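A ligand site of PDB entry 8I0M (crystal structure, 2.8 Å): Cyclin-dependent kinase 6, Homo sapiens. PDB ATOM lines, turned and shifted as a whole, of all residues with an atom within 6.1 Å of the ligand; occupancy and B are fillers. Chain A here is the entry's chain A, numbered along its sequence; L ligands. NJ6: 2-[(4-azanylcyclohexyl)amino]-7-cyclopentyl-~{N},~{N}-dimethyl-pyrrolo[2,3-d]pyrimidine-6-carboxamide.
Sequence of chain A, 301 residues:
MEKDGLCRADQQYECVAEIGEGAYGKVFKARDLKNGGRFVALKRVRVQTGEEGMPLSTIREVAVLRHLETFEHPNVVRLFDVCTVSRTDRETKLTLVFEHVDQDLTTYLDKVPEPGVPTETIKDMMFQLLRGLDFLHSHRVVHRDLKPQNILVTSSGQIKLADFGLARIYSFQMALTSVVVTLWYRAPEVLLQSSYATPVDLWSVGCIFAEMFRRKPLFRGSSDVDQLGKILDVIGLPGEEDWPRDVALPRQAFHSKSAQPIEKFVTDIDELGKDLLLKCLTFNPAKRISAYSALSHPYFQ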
ATOM      1  N   ILE A  19      30.281  28.423  -0.971  1.00  0.00           N
ATOM      2  CA  ILE A  19      29.779  27.107  -1.443  1.00  0.00           C
ATOM      3  C   ILE A  19      29.516  27.255  -2.936  1.00  0.00           C
ATOM      4  O   ILE A  19      29.983  26.405  -3.712  1.00  0.00           O
ATOM      5  CB  ILE A  19      28.551  26.690  -0.632  1.00  0.00           C
ATOM      6  CG1 ILE A  19      28.907  26.472   0.846  1.00  0.00           C
ATOM      7  CG2 ILE A  19      27.903  25.448  -1.246  1.00  0.00           C
ATOM      8  CD1 ILE A  19      27.784  26.757   1.812  1.00  0.00           C
ATOM      9  N   GLU A  21      26.432  28.735  -5.665  1.00  0.00           N
ATOM     10  CA  GLU A  21      25.087  29.231  -6.053  1.00  0.00           C
ATOM     11  C   GLU A  21      25.233  30.678  -6.551  1.00  0.00           C
ATOM     12  O   GLU A  21      25.506  30.840  -7.753  1.00  0.00           O
ATOM     13  CB  GLU A  21      24.098  29.106  -4.882  1.00  0.00           C
ATOM     14  N   VAL A  27      26.200  32.215  -0.758  1.00  0.00           N
ATOM     15  CA  VAL A  27      26.134  31.266   0.381  1.00  0.00           C
ATOM     16  C   VAL A  27      27.574  30.981   0.827  1.00  0.00           C
ATOM     17  O   VAL A  27      28.406  30.670  -0.027  1.00  0.00           O
ATOM     18  CB  VAL A  27      25.371  29.966   0.017  1.00  0.00           C
ATOM     19  CG1 VAL A  27      23.914  30.260  -0.281  1.00  0.00           C
ATOM     20  CG2 VAL A  27      25.989  29.233  -1.155  1.00  0.00           C
ATOM     21  N   ALA A  41      26.305  26.709   7.161  1.00  0.00           N
ATOM     22  CA  ALA A  41      26.053  27.383   5.872  1.00  0.00           C
ATOM     23  C   ALA A  41      25.292  28.684   6.142  1.00  0.00           C
ATOM     24  O   ALA A  41      24.236  28.614   6.797  1.00  0.00           O
ATOM     25  CB  ALA A  41      25.284  26.450   4.964  1.00  0.00           C
ATOM     26  N   LEU A  42      25.849  29.830   5.705  1.00  0.00           N
ATOM     27  CA  LEU A  42      25.224  31.180   5.785  1.00  0.00           C
ATOM     28  C   LEU A  42      24.734  31.628   4.405  1.00  0.00           C
ATOM     29  O   LEU A  42      25.470  31.409   3.422  1.00  0.00           O
ATOM     30  CB  LEU A  42      26.234  32.208   6.294  1.00  0.00           C
ATOM     31  CG  LEU A  42      26.807  31.954   7.681  1.00  0.00           C
ATOM     32  CD1 LEU A  42      27.298  33.263   8.287  1.00  0.00           C
ATOM     33  CD2 LEU A  42      25.779  31.301   8.602  1.00  0.00           C
ATOM     34  N   LYS A  43      23.564  32.238   4.366  1.00  0.00           N
ATOM     35  CA  LYS A  43      23.007  32.893   3.158  1.00  0.00           C
ATOM     36  C   LYS A  43      22.526  34.261   3.599  1.00  0.00           C
ATOM     37  O   LYS A  43      21.466  34.354   4.228  1.00  0.00           O
ATOM     38  CB  LYS A  43      21.866  32.079   2.527  1.00  0.00           C
ATOM     39  CG  LYS A  43      21.396  32.580   1.162  1.00  0.00           C
ATOM     40  CD  LYS A  43      19.943  32.250   0.872  1.00  0.00           C
ATOM     41  CE  LYS A  43      19.590  32.196  -0.607  1.00  0.00           C
ATOM     42  NZ  LYS A  43      18.254  31.598  -0.834  1.00  0.00           N
ATOM     43  N   VAL A  77      17.198  19.900   6.237  1.00  0.00           N
ATOM     44  CA  VAL A  77      18.364  20.589   6.853  1.00  0.00           C
ATOM     45  C   VAL A  77      17.842  21.458   7.999  1.00  0.00           C
ATOM     46  O   VAL A  77      16.764  22.000   7.874  1.00  0.00           O
ATOM     47  CB  VAL A  77      19.119  21.402   5.786  1.00  0.00           C
ATOM     48  CG1 VAL A  77      18.320  22.606   5.326  1.00  0.00           C
ATOM     49  CG2 VAL A  77      20.481  21.842   6.276  1.00  0.00           C
ATOM     50  N   LEU A  96      20.793  33.965   7.180  1.00  0.00           N
ATOM     51  CA  LEU A  96      20.197  32.668   7.587  1.00  0.00           C
ATOM     52  C   LEU A  96      21.302  31.669   7.905  1.00  0.00           C
ATOM     53  O   LEU A  96      22.221  31.519   7.087  1.00  0.00           O
ATOM     54  CB  LEU A  96      19.332  32.145   6.436  1.00  0.00           C
ATOM     55  CG  LEU A  96      17.870  32.545   6.499  1.00  0.00           C
ATOM     56  CD1 LEU A  96      17.713  34.047   6.609  1.00  0.00           C
ATOM     57  CD2 LEU A  96      17.123  31.998   5.286  1.00  0.00           C
ATOM     58  N   PHE A  98      22.252  27.776   8.630  1.00  0.00           N
ATOM     59  CA  PHE A  98      21.893  26.355   8.537  1.00  0.00           C
ATOM     60  C   PHE A  98      23.071  25.528   9.024  1.00  0.00           C
ATOM     61  O   PHE A  98      24.218  25.994   8.936  1.00  0.00           O
ATOM     62  CB  PHE A  98      21.595  25.932   7.094  1.00  0.00           C
ATOM     63  CG  PHE A  98      20.434  26.663   6.511  1.00  0.00           C
ATOM     64  CD1 PHE A  98      20.586  27.932   5.968  1.00  0.00           C
ATOM     65  CD2 PHE A  98      19.158  26.122   6.577  1.00  0.00           C
ATOM     66  CE1 PHE A  98      19.492  28.624   5.488  1.00  0.00           C
ATOM     67  CE2 PHE A  98      18.067  26.820   6.090  1.00  0.00           C
ATOM     68  CZ  PHE A  98      18.236  28.074   5.542  1.00  0.00           C
ATOM     69  N   GLU A  99      22.792  24.323   9.485  1.00  0.00           N
ATOM     70  CA  GLU A  99      23.836  23.305   9.559  1.00  0.00           C
ATOM     71  C   GLU A  99      24.458  23.171   8.168  1.00  0.00           C
ATOM     72  O   GLU A  99      23.747  23.393   7.192  1.00  0.00           O
ATOM     73  CB  GLU A  99      23.279  21.973  10.044  1.00  0.00           C
ATOM     74  CG  GLU A  99      22.061  21.496   9.274  1.00  0.00           C
ATOM     75  CD  GLU A  99      21.813  20.012   9.446  1.00  0.00           C
ATOM     76  OE1 GLU A  99      22.781  19.289   9.710  1.00  0.00           O
ATOM     77  OE2 GLU A  99      20.655  19.573   9.303  1.00  0.00           O
ATOM     78  N   HIS A 100      25.737  22.818   8.137  1.00  0.00           N
ATOM     79  CA  HIS A 100      26.515  22.495   6.934  1.00  0.00           C
ATOM     80  C   HIS A 100      26.571  20.976   6.783  1.00  0.00           C
ATOM     81  O   HIS A 100      26.838  20.290   7.775  1.00  0.00           O
ATOM     82  CB  HIS A 100      27.899  23.092   7.053  1.00  0.00           C
ATOM     83  CG  HIS A 100      28.790  22.617   5.975  1.00  0.00           C
ATOM     84  ND1 HIS A 100      28.558  22.922   4.661  1.00  0.00           N
ATOM     85  CD2 HIS A 100      29.888  21.838   6.008  1.00  0.00           C
ATOM     86  CE1 HIS A 100      29.485  22.358   3.918  1.00  0.00           C
ATOM     87  NE2 HIS A 100      30.300  21.683   4.718  1.00  0.00           N
ATOM     88  N   VAL A 101      26.329  20.481   5.585  1.00  0.00           N
ATOM     89  CA  VAL A 101      26.566  19.070   5.191  1.00  0.00           C
ATOM     90  C   VAL A 101      27.617  19.112   4.094  1.00  0.00           C
ATOM     91  O   VAL A 101      27.457  19.912   3.164  1.00  0.00           O
ATOM     92  CB  VAL A 101      25.281  18.405   4.709  1.00  0.00           C
ATOM     93  CG1 VAL A 101      25.502  16.954   4.299  1.00  0.00           C
ATOM     94  CG2 VAL A 101      24.166  18.524   5.729  1.00  0.00           C
ATOM     95  N   ASP A 102      28.662  18.315   4.214  1.00  0.00           N
ATOM     96  CA  ASP A 102      29.873  18.419   3.351  1.00  0.00           C
ATOM     97  C   ASP A 102      29.496  17.927   1.949  1.00  0.00           C
ATOM     98  O   ASP A 102      30.191  18.309   0.991  1.00  0.00           O
ATOM     99  CB  ASP A 102      31.061  17.652   3.945  1.00  0.00           C
ATOM    100  CG  ASP A 102      31.875  18.463   4.940  1.00  0.00           C
ATOM    101  OD1 ASP A 102      32.768  19.219   4.512  1.00  0.00           O
ATOM    102  OD2 ASP A 102      31.608  18.344   6.156  1.00  0.00           O
ATOM    103  N   GLN A 103      28.416  17.146   1.839  1.00  0.00           N
ATOM    104  CA  GLN A 103      28.184  16.301   0.658  1.00  0.00           C
ATOM    105  C   GLN A 103      26.765  16.502   0.117  1.00  0.00           C
ATOM    106  O   GLN A 103      25.846  16.768   0.910  1.00  0.00           O
ATOM    107  CB  GLN A 103      28.397  14.828   1.018  1.00  0.00           C
ATOM    108  CG  GLN A 103      28.938  14.021  -0.148  1.00  0.00           C
ATOM    109  CD  GLN A 103      28.753  12.539   0.046  1.00  0.00           C
ATOM    110  OE1 GLN A 103      28.338  12.080   1.115  1.00  0.00           O
ATOM    111  NE2 GLN A 103      29.049  11.770  -0.982  1.00  0.00           N
ATOM    112  N   ASP A 104      26.615  16.357  -1.205  1.00  0.00           N
ATOM    113  CA  ASP A 104      25.296  16.360  -1.892  1.00  0.00           C
ATOM    114  C   ASP A 104      25.137  15.037  -2.640  1.00  0.00           C
ATOM    115  O   ASP A 104      26.060  14.211  -2.600  1.00  0.00           O
ATOM    116  CB  ASP A 104      25.155  17.559  -2.822  1.00  0.00           C
ATOM    117  CG  ASP A 104      26.159  17.584  -3.946  1.00  0.00           C
ATOM    118  OD1 ASP A 104      26.701  16.524  -4.258  1.00  0.00           O
ATOM    119  OD2 ASP A 104      26.365  18.668  -4.500  1.00  0.00           O
ATOM    120  N   THR A 107      27.698  14.437  -5.649  1.00  0.00           N
ATOM    121  CA  THR A 107      29.057  14.034  -5.226  1.00  0.00           C
ATOM    122  C   THR A 107      29.014  12.590  -4.757  1.00  0.00           C
ATOM    123  O   THR A 107      30.020  11.882  -4.944  1.00  0.00           O
ATOM    124  CB  THR A 107      29.648  14.921  -4.134  1.00  0.00           C
ATOM    125  OG1 THR A 107      29.290  16.268  -4.397  1.00  0.00           O
ATOM    126  CG2 THR A 107      31.150  14.801  -4.091  1.00  0.00           C
ATOM    127  N   GLN A 149      21.599  18.743  -6.305  1.00  0.00           N
ATOM    128  CA  GLN A 149      22.609  19.695  -5.794  1.00  0.00           C
ATOM    129  C   GLN A 149      22.098  20.331  -4.506  1.00  0.00           C
ATOM    130  O   GLN A 149      22.939  20.783  -3.714  1.00  0.00           O
ATOM    131  CB  GLN A 149      22.938  20.751  -6.838  1.00  0.00           C
ATOM    132  CG  GLN A 149      23.696  20.206  -8.038  1.00  0.00           C
ATOM    133  CD  GLN A 149      22.825  19.958  -9.246  1.00  0.00           C
ATOM    134  OE1 GLN A 149      22.614  18.823  -9.669  1.00  0.00           O
ATOM    135  NE2 GLN A 149      22.321  21.046  -9.815  1.00  0.00           N
ATOM    136  N   ASN A 150      20.779  20.372  -4.302  1.00  0.00           N
ATOM    137  CA  ASN A 150      20.172  20.835  -3.023  1.00  0.00           C
ATOM    138  C   ASN A 150      19.534  19.652  -2.281  1.00  0.00           C
ATOM    139  O   ASN A 150      18.590  19.852  -1.518  1.00  0.00           O
ATOM    140  CB  ASN A 150      19.150  21.949  -3.261  1.00  0.00           C
ATOM    141  CG  ASN A 150      18.196  21.594  -4.363  1.00  0.00           C
ATOM    142  OD1 ASN A 150      17.687  20.475  -4.419  1.00  0.00           O
ATOM    143  ND2 ASN A 150      17.955  22.551  -5.251  1.00  0.00           N
ATOM    144  N   ILE A 151      20.028  18.449  -2.532  1.00  0.00           N
ATOM    145  CA  ILE A 151      19.762  17.272  -1.685  1.00  0.00           C
ATOM    146  C   ILE A 151      21.056  16.894  -0.964  1.00  0.00           C
ATOM    147  O   ILE A 151      22.034  16.545  -1.641  1.00  0.00           O
ATOM    148  CB  ILE A 151      19.245  16.122  -2.554  1.00  0.00           C
ATOM    149  CG1 ILE A 151      17.814  16.403  -2.999  1.00  0.00           C
ATOM    150  CG2 ILE A 151      19.376  14.810  -1.823  1.00  0.00           C
ATOM    151  CD1 ILE A 151      17.328  15.462  -4.069  1.00  0.00           C
ATOM    152  N   LEU A 152      21.062  16.962   0.369  1.00  0.00           N
ATOM    153  CA  LEU A 152      22.291  16.794   1.191  1.00  0.00           C
ATOM    154  C   LEU A 152      22.334  15.386   1.785  1.00  0.00           C
ATOM    155  O   LEU A 152      21.291  14.849   2.159  1.00  0.00           O
ATOM    156  CB  LEU A 152      22.287  17.875   2.272  1.00  0.00           C
ATOM    157  CG  LEU A 152      22.210  19.302   1.738  1.00  0.00           C
ATOM    158  CD1 LEU A 152      22.385  20.321   2.844  1.00  0.00           C
ATOM    159  CD2 LEU A 152      23.227  19.544   0.646  1.00  0.00           C
ATOM    160  N   LEU A 161      16.909  17.892   2.834  1.00  0.00           N
ATOM    161  CA  LEU A 161      16.483  18.826   1.780  1.00  0.00           C
ATOM    162  C   LEU A 161      16.948  20.239   2.116  1.00  0.00           C
ATOM    163  O   LEU A 161      16.907  20.585   3.316  1.00  0.00           O
ATOM    164  CB  LEU A 161      14.962  18.756   1.681  1.00  0.00           C
ATOM    165  CG  LEU A 161      14.441  17.366   1.351  1.00  0.00           C
ATOM    166  CD1 LEU A 161      13.059  17.424   0.740  1.00  0.00           C
ATOM    167  CD2 LEU A 161      15.402  16.641   0.417  1.00  0.00           C
ATOM    168  N   ALA A 162      17.296  21.010   1.082  1.00  0.00           N
ATOM    169  CA  ALA A 162      17.835  22.376   1.208  1.00  0.00           C
ATOM    170  C   ALA A 162      17.424  23.239  -0.007  1.00  0.00           C
ATOM    171  O   ALA A 162      16.956  22.672  -0.997  1.00  0.00           O
ATOM    172  CB  ALA A 162      19.332  22.277   1.357  1.00  0.00           C
ATOM    173  N   ASP A 163      17.569  24.564   0.146  1.00  0.00           N
ATOM    174  CA  ASP A 163      17.427  25.629  -0.880  1.00  0.00           C
ATOM    175  C   ASP A 163      15.982  25.649  -1.399  1.00  0.00           C
ATOM    176  O   ASP A 163      15.745  25.461  -2.632  1.00  0.00           O
ATOM    177  CB  ASP A 163      18.502  25.522  -1.971  1.00  0.00           C
ATOM    178  CG  ASP A 163      19.235  26.833  -2.218  1.00  0.00           C
ATOM    179  OD1 ASP A 163      18.735  27.908  -1.765  1.00  0.00           O
ATOM    180  OD2 ASP A 163      20.320  26.775  -2.844  1.00  0.00           O
ATOM    181  N   PHE A 164      15.057  25.897  -0.464  1.00  0.00           N
ATOM    182  CA  PHE A 164      13.595  25.999  -0.694  1.00  0.00           C
ATOM    183  C   PHE A 164      13.018  27.116   0.197  1.00  0.00           C
ATOM    184  O   PHE A 164      13.675  27.502   1.166  1.00  0.00           O
ATOM    185  CB  PHE A 164      12.964  24.615  -0.460  1.00  0.00           C
ATOM    186  CG  PHE A 164      12.981  24.182   0.971  1.00  0.00           C
ATOM    187  CD1 PHE A 164      11.985  24.578   1.844  1.00  0.00           C
ATOM    188  CD2 PHE A 164      14.016  23.414   1.481  1.00  0.00           C
ATOM    189  CE1 PHE A 164      12.027  24.222   3.185  1.00  0.00           C
ATOM    190  CE2 PHE A 164      14.058  23.059   2.821  1.00  0.00           C
ATOM    191  CZ  PHE A 164      13.064  23.478   3.673  1.00  0.00           C
HETATM  192  N1  NJ6 L   1      26.342  21.747   1.663  1.00  0.00           N
HETATM  193  N3  NJ6 L   1      24.527  23.139   1.429  1.00  0.00           N
HETATM  194  C4  NJ6 L   1      26.185  21.055  -0.661  1.00  0.00           C
HETATM  195  C5  NJ6 L   1      26.788  22.056   0.310  1.00  0.00           C
HETATM  196  C6  NJ6 L   1      28.295  22.077   0.208  1.00  0.00           C
HETATM  197  C7  NJ6 L   1      25.307  22.386   2.240  1.00  0.00           C
HETATM  198  C8  NJ6 L   1      23.524  23.769   2.060  1.00  0.00           C
HETATM  199  C10 NJ6 L   1      24.151  22.860   4.175  1.00  0.00           C
HETATM  200  C13 NJ6 L   1      22.447  25.004   0.093  1.00  0.00           C
HETATM  201  C15 NJ6 L   1      23.220  23.833  -1.890  1.00  0.00           C
HETATM  202  C17 NJ6 L   1      23.733  25.635  -0.472  1.00  0.00           C
HETATM  203  C20 NJ6 L   1      19.771  28.221   1.817  1.00  0.00           C
HETATM  204  C1  NJ6 L   1      28.830  20.842  -0.522  1.00  0.00           C
HETATM  205  C11 NJ6 L   1      21.711  25.006   2.508  1.00  0.00           C
HETATM  206  C12 NJ6 L   1      22.137  24.453   3.710  1.00  0.00           C
HETATM  207  C14 NJ6 L   1      22.114  23.848  -0.859  1.00  0.00           C
HETATM  208  C16 NJ6 L   1      23.733  25.238  -1.918  1.00  0.00           C
HETATM  209  C18 NJ6 L   1      20.620  25.944   2.215  1.00  0.00           C
HETATM  210  C19 NJ6 L   1      22.183  27.840   2.157  1.00  0.00           C
HETATM  211  C2  NJ6 L   1      28.304  20.784  -1.952  1.00  0.00           C
HETATM  212  C3  NJ6 L   1      26.846  21.172  -2.031  1.00  0.00           C
HETATM  213  C9  NJ6 L   1      23.288  23.670   3.430  1.00  0.00           C
HETATM  214  N2  NJ6 L   1      29.120  21.673  -2.828  1.00  0.00           N
HETATM  215  N4  NJ6 L   1      25.150  22.230   3.571  1.00  0.00           N
HETATM  216  N5  NJ6 L   1      22.575  24.594   1.503  1.00  0.00           N
HETATM  217  N6  NJ6 L   1      20.836  27.257   2.057  1.00  0.00           N
HETATM  218  O1  NJ6 L   1      19.489  25.501   2.097  1.00  0.00           O
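N of Val 101 sits at hydrogen-bond distance from N4 of the ligand, at 2.9 Å. The backbone NH of Asp 163 is in hydrogen-bond range of an oxygen (O1) of the ligand, 2.9 Å away. The backbone carbonyl oxygen (O) of Val 101 lies within hydrogen-bond range of a nitrogen (N1) of the ligand, 2.6 Å away.
Residues that only touch the ligand: Ile 19 (3.7 Å), Val 27 (3.8 Å), Ala 41 (3.8 Å), Phe 98 (3.7 Å), Glu 99 (3.1 Å), His 100 (3.6 Å), Asp 102 (3.2 Å), Asp 104 (3.5 Å), Gln 149 (3.6 Å), Leu 152 (3.4 Å) and Ala 162 (3.3 Å). Of the 24 residues printed, 13 come within 4 Å of the ligand. Along chain A the residues within 4 Å of the ligand span positions 19 to 163. The nearest printed residue that does not touch the ligand is Val 77 (4.02 Å).
OD1 of Asp 163 lies within salt-bridge range of NZ of Lys 43. The backbone NH of Ala 162 sits at hydrogen-bond distance from the backbone carbonyl oxygen of Asn 150 (3.1 Å). OG1 of Thr 107 is in hydrogen-bond range of OD1 of Asp 104 (2.6 Å). OD1 of Asp 102 lies within hydrogen-bond range of NE2 of His 100 (3.5 Å). The backbone carbonyl oxygen of Ala 41 is in hydrogen-bond range of the backbone NH of Phe 98, at 2.8 Å. N of Ile 19 lies within hydrogen-bond range of O of Val 27 (3.1 Å).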
